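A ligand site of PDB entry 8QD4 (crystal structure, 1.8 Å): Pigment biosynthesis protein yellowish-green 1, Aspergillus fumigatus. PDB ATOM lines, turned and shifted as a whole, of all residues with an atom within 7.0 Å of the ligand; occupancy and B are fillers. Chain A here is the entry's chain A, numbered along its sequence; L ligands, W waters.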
ATOM      1  N   TYR A  54      20.834 -10.652  11.053  1.00  0.00           N
ATOM      2  CA  TYR A  54      21.387 -12.031  11.008  1.00  0.00           C
ATOM      3  C   TYR A  54      20.233 -13.029  11.078  1.00  0.00           C
ATOM      4  O   TYR A  54      19.387 -12.908  11.956  1.00  0.00           O
ATOM      5  CB  TYR A  54      22.386 -12.276  12.139  1.00  0.00           C
ATOM      6  CG  TYR A  54      22.799 -13.729  12.224  1.00  0.00           C
ATOM      7  CD1 TYR A  54      23.853 -14.216  11.473  1.00  0.00           C
ATOM      8  CD2 TYR A  54      22.067 -14.624  12.983  1.00  0.00           C
ATOM      9  CE1 TYR A  54      24.206 -15.550  11.509  1.00  0.00           C
ATOM     10  CE2 TYR A  54      22.397 -15.964  13.024  1.00  0.00           C
ATOM     11  CZ  TYR A  54      23.469 -16.431  12.284  1.00  0.00           C
ATOM     12  OH  TYR A  54      23.807 -17.750  12.321  1.00  0.00           O
ATOM     13  N   PRO A  55      20.187 -14.064  10.203  1.00  0.00           N
ATOM     14  CA  PRO A  55      21.216 -14.299   9.179  1.00  0.00           C
ATOM     15  C   PRO A  55      20.940 -13.737   7.772  1.00  0.00           C
ATOM     16  O   PRO A  55      21.649 -14.116   6.851  1.00  0.00           O
ATOM     17  CB  PRO A  55      21.206 -15.838   9.151  1.00  0.00           C
ATOM     18  CG  PRO A  55      19.729 -16.178   9.267  1.00  0.00           C
ATOM     19  CD  PRO A  55      19.184 -15.131  10.225  1.00  0.00           C
ATOM     20  N   PHE A 127      22.345 -22.846   4.746  1.00  0.00           N
ATOM     21  CA  PHE A 127      22.235 -22.888   6.223  1.00  0.00           C
ATOM     22  C   PHE A 127      21.872 -24.329   6.618  1.00  0.00           C
ATOM     23  O   PHE A 127      21.065 -24.954   5.909  1.00  0.00           O
ATOM     24  CB  PHE A 127      21.123 -21.940   6.691  1.00  0.00           C
ATOM     25  CG  PHE A 127      21.170 -21.555   8.147  1.00  0.00           C
ATOM     26  CD1 PHE A 127      21.858 -20.422   8.556  1.00  0.00           C
ATOM     27  CD2 PHE A 127      20.530 -22.309   9.107  1.00  0.00           C
ATOM     28  CE1 PHE A 127      21.926 -20.073   9.885  1.00  0.00           C
ATOM     29  CE2 PHE A 127      20.592 -21.960  10.452  1.00  0.00           C
ATOM     30  CZ  PHE A 127      21.290 -20.841  10.829  1.00  0.00           C
ATOM     31  N   THR A 202      35.333 -16.634  11.331  1.00  0.00           N
ATOM     32  CA  THR A 202      33.890 -16.869  11.076  1.00  0.00           C
ATOM     33  C   THR A 202      33.459 -18.122  11.848  1.00  0.00           C
ATOM     34  O   THR A 202      34.299 -18.705  12.544  1.00  0.00           O
ATOM     35  CB  THR A 202      33.613 -16.958   9.568  1.00  0.00           C
ATOM     36  OG1 THR A 202      34.526 -17.867   8.973  1.00  0.00           O
ATOM     37  CG2 THR A 202      33.699 -15.606   8.885  1.00  0.00           C
ATOM     38  N   GLY A 203      32.187 -18.520  11.720  1.00  0.00           N
ATOM     39  CA  GLY A 203      31.596 -19.597  12.528  1.00  0.00           C
ATOM     40  C   GLY A 203      31.054 -20.747  11.698  1.00  0.00           C
ATOM     41  O   GLY A 203      31.638 -21.045  10.614  1.00  0.00           O
ATOM     42  N   LEU A 204      30.018 -21.410  12.208  1.00  0.00           N
ATOM     43  CA  LEU A 204      29.526 -22.707  11.688  1.00  0.00           C
ATOM     44  C   LEU A 204      28.782 -22.476  10.366  1.00  0.00           C
ATOM     45  O   LEU A 204      28.986 -23.289   9.453  1.00  0.00           O
ATOM     46  CB  LEU A 204      28.620 -23.369  12.729  1.00  0.00           C
ATOM     47  CG  LEU A 204      28.025 -24.716  12.314  1.00  0.00           C
ATOM     48  CD1 LEU A 204      29.115 -25.777  12.222  1.00  0.00           C
ATOM     49  CD2 LEU A 204      26.931 -25.142  13.270  1.00  0.00           C
ATOM     50  N   ASP A 205      27.965 -21.422  10.281  1.00  0.00           N
ATOM     51  CA  ASP A 205      27.001 -21.167   9.174  1.00  0.00           C
ATOM     52  C   ASP A 205      27.321 -19.855   8.448  1.00  0.00           C
ATOM     53  O   ASP A 205      26.622 -19.551   7.465  1.00  0.00           O
ATOM     54  CB  ASP A 205      25.568 -21.087   9.701  1.00  0.00           C
ATOM     55  CG  ASP A 205      25.394 -20.107  10.836  1.00  0.00           C
ATOM     56  OD1 ASP A 205      25.449 -18.890  10.581  1.00  0.00           O
ATOM     57  OD2 ASP A 205      25.210 -20.574  11.972  1.00  0.00           O
ATOM     58  N   GLY A 206      28.308 -19.095   8.943  1.00  0.00           N
ATOM     59  CA  GLY A 206      28.703 -17.783   8.384  1.00  0.00           C
ATOM     60  C   GLY A 206      30.161 -17.830   7.976  1.00  0.00           C
ATOM     61  O   GLY A 206      30.994 -18.144   8.828  1.00  0.00           O
ATOM     62  N   ILE A 230      37.158 -20.956  10.034  1.00  0.00           N
ATOM     63  CA  ILE A 230      37.726 -21.718  11.177  1.00  0.00           C
ATOM     64  C   ILE A 230      37.915 -23.179  10.770  1.00  0.00           C
ATOM     65  O   ILE A 230      37.267 -23.659   9.825  1.00  0.00           O
ATOM     66  CB  ILE A 230      36.844 -21.588  12.434  1.00  0.00           C
ATOM     67  CG1 ILE A 230      35.373 -21.878  12.146  1.00  0.00           C
ATOM     68  CG2 ILE A 230      37.027 -20.231  13.086  1.00  0.00           C
ATOM     69  CD1 ILE A 230      34.585 -22.302  13.364  1.00  0.00           C
ATOM     70  N   LEU A 273      33.340 -14.934  15.827  1.00  0.00           N
ATOM     71  CA  LEU A 273      31.873 -14.878  15.986  1.00  0.00           C
ATOM     72  C   LEU A 273      31.327 -16.295  16.156  1.00  0.00           C
ATOM     73  O   LEU A 273      31.775 -17.165  15.411  1.00  0.00           O
ATOM     74  CB  LEU A 273      31.292 -14.277  14.708  1.00  0.00           C
ATOM     75  CG  LEU A 273      32.006 -13.020  14.191  1.00  0.00           C
ATOM     76  CD1 LEU A 273      31.654 -12.742  12.746  1.00  0.00           C
ATOM     77  CD2 LEU A 273      31.671 -11.827  15.073  1.00  0.00           C
ATOM     78  N   SER A 274      30.437 -16.483  17.129  1.00  0.00           N
ATOM     79  CA  SER A 274      29.796 -17.786  17.287  1.00  0.00           C
ATOM     80  C   SER A 274      30.826 -18.922  17.450  1.00  0.00           C
ATOM     81  O   SER A 274      31.518 -18.970  18.417  1.00  0.00           O
ATOM     82  CB  SER A 274      28.801 -18.053  16.169  1.00  0.00           C
ATOM     83  OG  SER A 274      27.844 -19.027  16.567  1.00  0.00           O
ATOM     84  N   ALA A 275      30.835 -19.854  16.507  1.00  0.00           N
ATOM     85  CA  ALA A 275      31.798 -20.976  16.511  1.00  0.00           C
ATOM     86  C   ALA A 275      33.217 -20.411  16.424  1.00  0.00           C
ATOM     87  O   ALA A 275      34.161 -21.101  16.809  1.00  0.00           O
ATOM     88  CB  ALA A 275      31.510 -21.940  15.394  1.00  0.00           C
ATOM     89  N   GLY A 276      33.351 -19.248  15.781  1.00  0.00           N
ATOM     90  CA  GLY A 276      34.648 -18.552  15.690  1.00  0.00           C
ATOM     91  C   GLY A 276      35.140 -18.118  17.058  1.00  0.00           C
ATOM     92  O   GLY A 276      36.342 -17.940  17.209  1.00  0.00           O
ATOM     93  N   HIS A 297      32.687 -13.493  20.374  1.00  0.00           N
ATOM     94  CA  HIS A 297      31.230 -13.181  20.396  1.00  0.00           C
ATOM     95  C   HIS A 297      30.433 -14.486  20.503  1.00  0.00           C
ATOM     96  O   HIS A 297      30.512 -15.275  19.557  1.00  0.00           O
ATOM     97  CB  HIS A 297      30.885 -12.458  19.095  1.00  0.00           C
ATOM     98  CG  HIS A 297      30.100 -11.210  19.280  1.00  0.00           C
ATOM     99  ND1 HIS A 297      30.556  -9.989  18.844  1.00  0.00           N
ATOM    100  CD2 HIS A 297      28.892 -10.993  19.842  1.00  0.00           C
ATOM    101  CE1 HIS A 297      29.662  -9.073  19.133  1.00  0.00           C
ATOM    102  NE2 HIS A 297      28.631  -9.665  19.741  1.00  0.00           N
ATOM    103  N   GLY A 298      29.655 -14.648  21.572  1.00  0.00           N
ATOM    104  CA  GLY A 298      28.869 -15.883  21.761  1.00  0.00           C
ATOM    105  C   GLY A 298      29.759 -17.105  21.662  1.00  0.00           C
ATOM    106  O   GLY A 298      29.499 -17.937  20.803  1.00  0.00           O
ATOM    107  N   TYR A 318      18.871 -22.513  18.229  1.00  0.00           N
ATOM    108  CA  TYR A 318      19.448 -22.702  16.864  1.00  0.00           C
ATOM    109  C   TYR A 318      18.311 -22.994  15.880  1.00  0.00           C
ATOM    110  O   TYR A 318      17.431 -23.810  16.186  1.00  0.00           O
ATOM    111  CB  TYR A 318      20.574 -23.731  16.833  1.00  0.00           C
ATOM    112  CG  TYR A 318      21.494 -23.474  15.672  1.00  0.00           C
ATOM    113  CD1 TYR A 318      22.353 -22.395  15.690  1.00  0.00           C
ATOM    114  CD2 TYR A 318      21.427 -24.221  14.512  1.00  0.00           C
ATOM    115  CE1 TYR A 318      23.177 -22.095  14.623  1.00  0.00           C
ATOM    116  CE2 TYR A 318      22.237 -23.949  13.428  1.00  0.00           C
ATOM    117  CZ  TYR A 318      23.113 -22.879  13.483  1.00  0.00           C
ATOM    118  OH  TYR A 318      23.924 -22.585  12.436  1.00  0.00           O
ATOM    119  N   PRO A 319      18.309 -22.391  14.675  1.00  0.00           N
ATOM    120  CA  PRO A 319      17.177 -22.549  13.745  1.00  0.00           C
ATOM    121  C   PRO A 319      16.848 -23.981  13.311  1.00  0.00           C
ATOM    122  O   PRO A 319      15.693 -24.232  13.038  1.00  0.00           O
ATOM    123  CB  PRO A 319      17.616 -21.734  12.514  1.00  0.00           C
ATOM    124  CG  PRO A 319      18.555 -20.700  13.084  1.00  0.00           C
ATOM    125  CD  PRO A 319      19.311 -21.442  14.159  1.00  0.00           C
ATOM    126  N   ILE A 322      21.869 -28.944  15.226  1.00  0.00           N
ATOM    127  CA  ILE A 322      23.264 -28.399  15.192  1.00  0.00           C
ATOM    128  C   ILE A 322      24.315 -29.480  15.503  1.00  0.00           C
ATOM    129  O   ILE A 322      25.487 -29.262  15.127  1.00  0.00           O
ATOM    130  CB  ILE A 322      23.393 -27.187  16.142  1.00  0.00           C
ATOM    131  CG1 ILE A 322      24.591 -26.311  15.765  1.00  0.00           C
ATOM    132  CG2 ILE A 322      23.444 -27.604  17.606  1.00  0.00           C
ATOM    133  CD1 ILE A 322      24.639 -24.978  16.487  1.00  0.00           C
ATOM    134  N   TRP A 326      28.159 -29.881  14.131  1.00  0.00           N
ATOM    135  CA  TRP A 326      29.223 -29.761  15.166  1.00  0.00           C
ATOM    136  C   TRP A 326      30.161 -30.980  15.072  1.00  0.00           C
ATOM    137  O   TRP A 326      31.374 -30.752  14.900  1.00  0.00           O
ATOM    138  CB  TRP A 326      28.609 -29.604  16.568  1.00  0.00           C
ATOM    139  CG  TRP A 326      28.219 -28.198  16.916  1.00  0.00           C
ATOM    140  CD1 TRP A 326      28.191 -27.113  16.088  1.00  0.00           C
ATOM    141  CD2 TRP A 326      27.805 -27.724  18.210  1.00  0.00           C
ATOM    142  NE1 TRP A 326      27.803 -25.999  16.781  1.00  0.00           N
ATOM    143  CE2 TRP A 326      27.548 -26.340  18.085  1.00  0.00           C
ATOM    144  CE3 TRP A 326      27.620 -28.333  19.459  1.00  0.00           C
ATOM    145  CZ2 TRP A 326      27.109 -25.557  19.147  1.00  0.00           C
ATOM    146  CZ3 TRP A 326      27.198 -27.559  20.510  1.00  0.00           C
ATOM    147  CH2 TRP A 326      26.957 -26.190  20.360  1.00  0.00           C
ATOM    148  N   VAL A 371      22.579 -22.353  22.771  1.00  0.00           N
ATOM    149  CA  VAL A 371      23.541 -22.980  21.818  1.00  0.00           C
ATOM    150  C   VAL A 371      24.823 -23.324  22.587  1.00  0.00           C
ATOM    151  O   VAL A 371      25.171 -24.516  22.624  1.00  0.00           O
ATOM    152  CB  VAL A 371      23.802 -22.059  20.607  1.00  0.00           C
ATOM    153  CG1 VAL A 371      24.739 -22.712  19.597  1.00  0.00           C
ATOM    154  CG2 VAL A 371      22.515 -21.623  19.933  1.00  0.00           C
ATOM    155  N   VAL A 372      25.492 -22.339  23.196  1.00  0.00           N
ATOM    156  CA  VAL A 372      26.692 -22.556  24.067  1.00  0.00           C
ATOM    157  C   VAL A 372      26.432 -21.896  25.412  1.00  0.00           C
ATOM    158  O   VAL A 372      25.836 -20.826  25.479  1.00  0.00           O
ATOM    159  CB  VAL A 372      27.997 -22.014  23.436  1.00  0.00           C
ATOM    160  CG1 VAL A 372      28.402 -22.800  22.190  1.00  0.00           C
ATOM    161  CG2 VAL A 372      27.912 -20.530  23.149  1.00  0.00           C
ATOM    162  N   HIS A 397      21.648 -16.739  22.148  1.00  0.00           N
ATOM    163  CA  HIS A 397      23.027 -16.842  21.596  1.00  0.00           C
ATOM    164  C   HIS A 397      23.383 -15.590  20.780  1.00  0.00           C
ATOM    165  O   HIS A 397      22.552 -15.184  19.956  1.00  0.00           O
ATOM    166  CB  HIS A 397      23.093 -18.063  20.668  1.00  0.00           C
ATOM    167  CG  HIS A 397      24.452 -18.413  20.151  1.00  0.00           C
ATOM    168  ND1 HIS A 397      25.546 -18.514  20.970  1.00  0.00           N
ATOM    169  CD2 HIS A 397      24.879 -18.725  18.919  1.00  0.00           C
ATOM    170  CE1 HIS A 397      26.587 -18.858  20.259  1.00  0.00           C
ATOM    171  NE2 HIS A 397      26.212 -18.991  18.999  1.00  0.00           N
ATOM    172  N   MET A 398      24.541 -15.006  21.132  1.00  0.00           N
ATOM    173  CA  MET A 398      25.268 -13.814  20.579  1.00  0.00           C
ATOM    174  C   MET A 398      24.746 -12.511  21.195  1.00  0.00           C
ATOM    175  O   MET A 398      25.417 -11.480  21.036  1.00  0.00           O
ATOM    176  CB  MET A 398      25.211 -13.687  19.052  1.00  0.00           C
ATOM    177  CG  MET A 398      25.611 -14.929  18.318  1.00  0.00           C
ATOM    178  SD  MET A 398      27.384 -15.139  18.339  1.00  0.00           S
ATOM    179  CE  MET A 398      27.886 -13.819  17.242  1.00  0.00           C
ATOM    180  N   GLY A 399      23.581 -12.540  21.845  1.00  0.00           N
ATOM    181  CA  GLY A 399      22.983 -11.323  22.423  1.00  0.00           C
ATOM    182  C   GLY A 399      22.850 -10.186  21.416  1.00  0.00           C
ATOM    183  O   GLY A 399      23.208  -9.053  21.775  1.00  0.00           O
ATOM    184  N   TYR A 400      22.445 -10.472  20.179  1.00  0.00           N
ATOM    185  CA  TYR A 400      22.209  -9.397  19.179  1.00  0.00           C
ATOM    186  C   TYR A 400      20.832  -8.782  19.505  1.00  0.00           C
ATOM    187  O   TYR A 400      20.007  -9.484  20.109  1.00  0.00           O
ATOM    188  CB  TYR A 400      22.295  -9.922  17.731  1.00  0.00           C
ATOM    189  CG  TYR A 400      23.676 -10.216  17.191  1.00  0.00           C
ATOM    190  CD1 TYR A 400      23.868 -11.185  16.228  1.00  0.00           C
ATOM    191  CD2 TYR A 400      24.796  -9.530  17.625  1.00  0.00           C
ATOM    192  CE1 TYR A 400      25.121 -11.477  15.715  1.00  0.00           C
ATOM    193  CE2 TYR A 400      26.056  -9.801  17.133  1.00  0.00           C
ATOM    194  CZ  TYR A 400      26.224 -10.782  16.162  1.00  0.00           C
ATOM    195  OH  TYR A 400      27.467 -11.052  15.669  1.00  0.00           O
HETATM  196  C1  LIG L   1      26.642 -18.795  14.197  1.00  0.00           C
HETATM  197  S1  LIG L   1      27.237 -19.929  15.445  1.00  0.00           S
HETATM  198  C2  LIG L   1      25.755 -17.710  14.749  1.00  0.00           C
HETATM  199  C3  LIG L   1      24.573 -18.021  15.381  1.00  0.00           C
HETATM  200  C4  LIG L   1      23.755 -17.020  15.880  1.00  0.00           C
HETATM  201  C5  LIG L   1      24.119 -15.701  15.733  1.00  0.00           C
HETATM  202  C6  LIG L   1      25.301 -15.383  15.113  1.00  0.00           C
HETATM  203  C7  LIG L   1      26.125 -16.385  14.623  1.00  0.00           C
HETATM  204  O1  LIG L   1      26.145 -20.644  16.002  1.00  0.00           O
HETATM  205  O2  LIG L   1      28.308 -20.617  14.863  1.00  0.00           O
HETATM  206  O   HOH W   1      27.755 -15.405  12.061  1.00  0.00           O
HETATM  207  O   HOH W   2      28.133 -23.079  16.222  1.00  0.00           O
HETATM  208  O   HOH W   3      28.686 -18.326  11.876  1.00  0.00           O
HETATM  209  O   HOH W   4      27.400 -21.788  18.302  1.00  0.00           O
HETATM  210  O   HOH W   5      21.639 -18.864  13.760  1.00  0.00           O
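The backbone NH (N) of Leu 204 is in hydrogen-bond range of an oxygen (O2) of the ligand (3.3 Å).
A sulfur (S1) of the ligand is covalently linked to the side-chain hydroxyl (OG) of Ser 274, at 1.6 Å.
The backbone NH (N) of Ala 275 is in hydrogen-bond range of an oxygen (O2) of the ligand (3.1 Å).
NE2 of His 397 lies within hydrogen-bond range of O1 of the ligand (3.4 Å).
The side-chain hydroxyl (OH) of Tyr 318 sits at hydrogen-bond distance from the side-chain carboxylate (OD2) of Asp 205, 2.4 Å away.
The side-chain hydroxyl of Ser 274 is in hydrogen-bond range of a ring nitrogen (NE2) of His 397.
N of Ser 274 sits at hydrogen-bond distance from SD of Met 398 (3.5 Å).
O of His 297 lies within hydrogen-bond range of N of Ser 274 (2.7 Å).
The side-chain carboxylate (OD1) of Asp 205 lies within hydrogen-bond range of the side-chain hydroxyl (OH) of Tyr 54.
Tyr 54 touches the ligand.
Asp 205 touches the ligand (OD2 to C1, 3.2 Å).
Tyr 318 touches the ligand.
CG of Met 398 touches C5 of the ligand, at 3.1 Å.
Tyr 400 touches the ligand.
Hydrophobic or aromatic side chains that line the ligand: Tyr 54, Leu 204, Ala 275, Tyr 318, His 397, Met 398 and Tyr 400.
Water W2 bridges an oxygen (O2) of the ligand (2.8 Å) and the indole nitrogen (NE1) of Trp 326 (3.0 Å).
Water W4 lies within hydrogen-bond range of an oxygen (O1) of the ligand (2.9 Å), a ring nitrogen (NE2) of His 397 (3.1 Å) and the side-chain hydroxyl of Ser 274 (3.3 Å).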
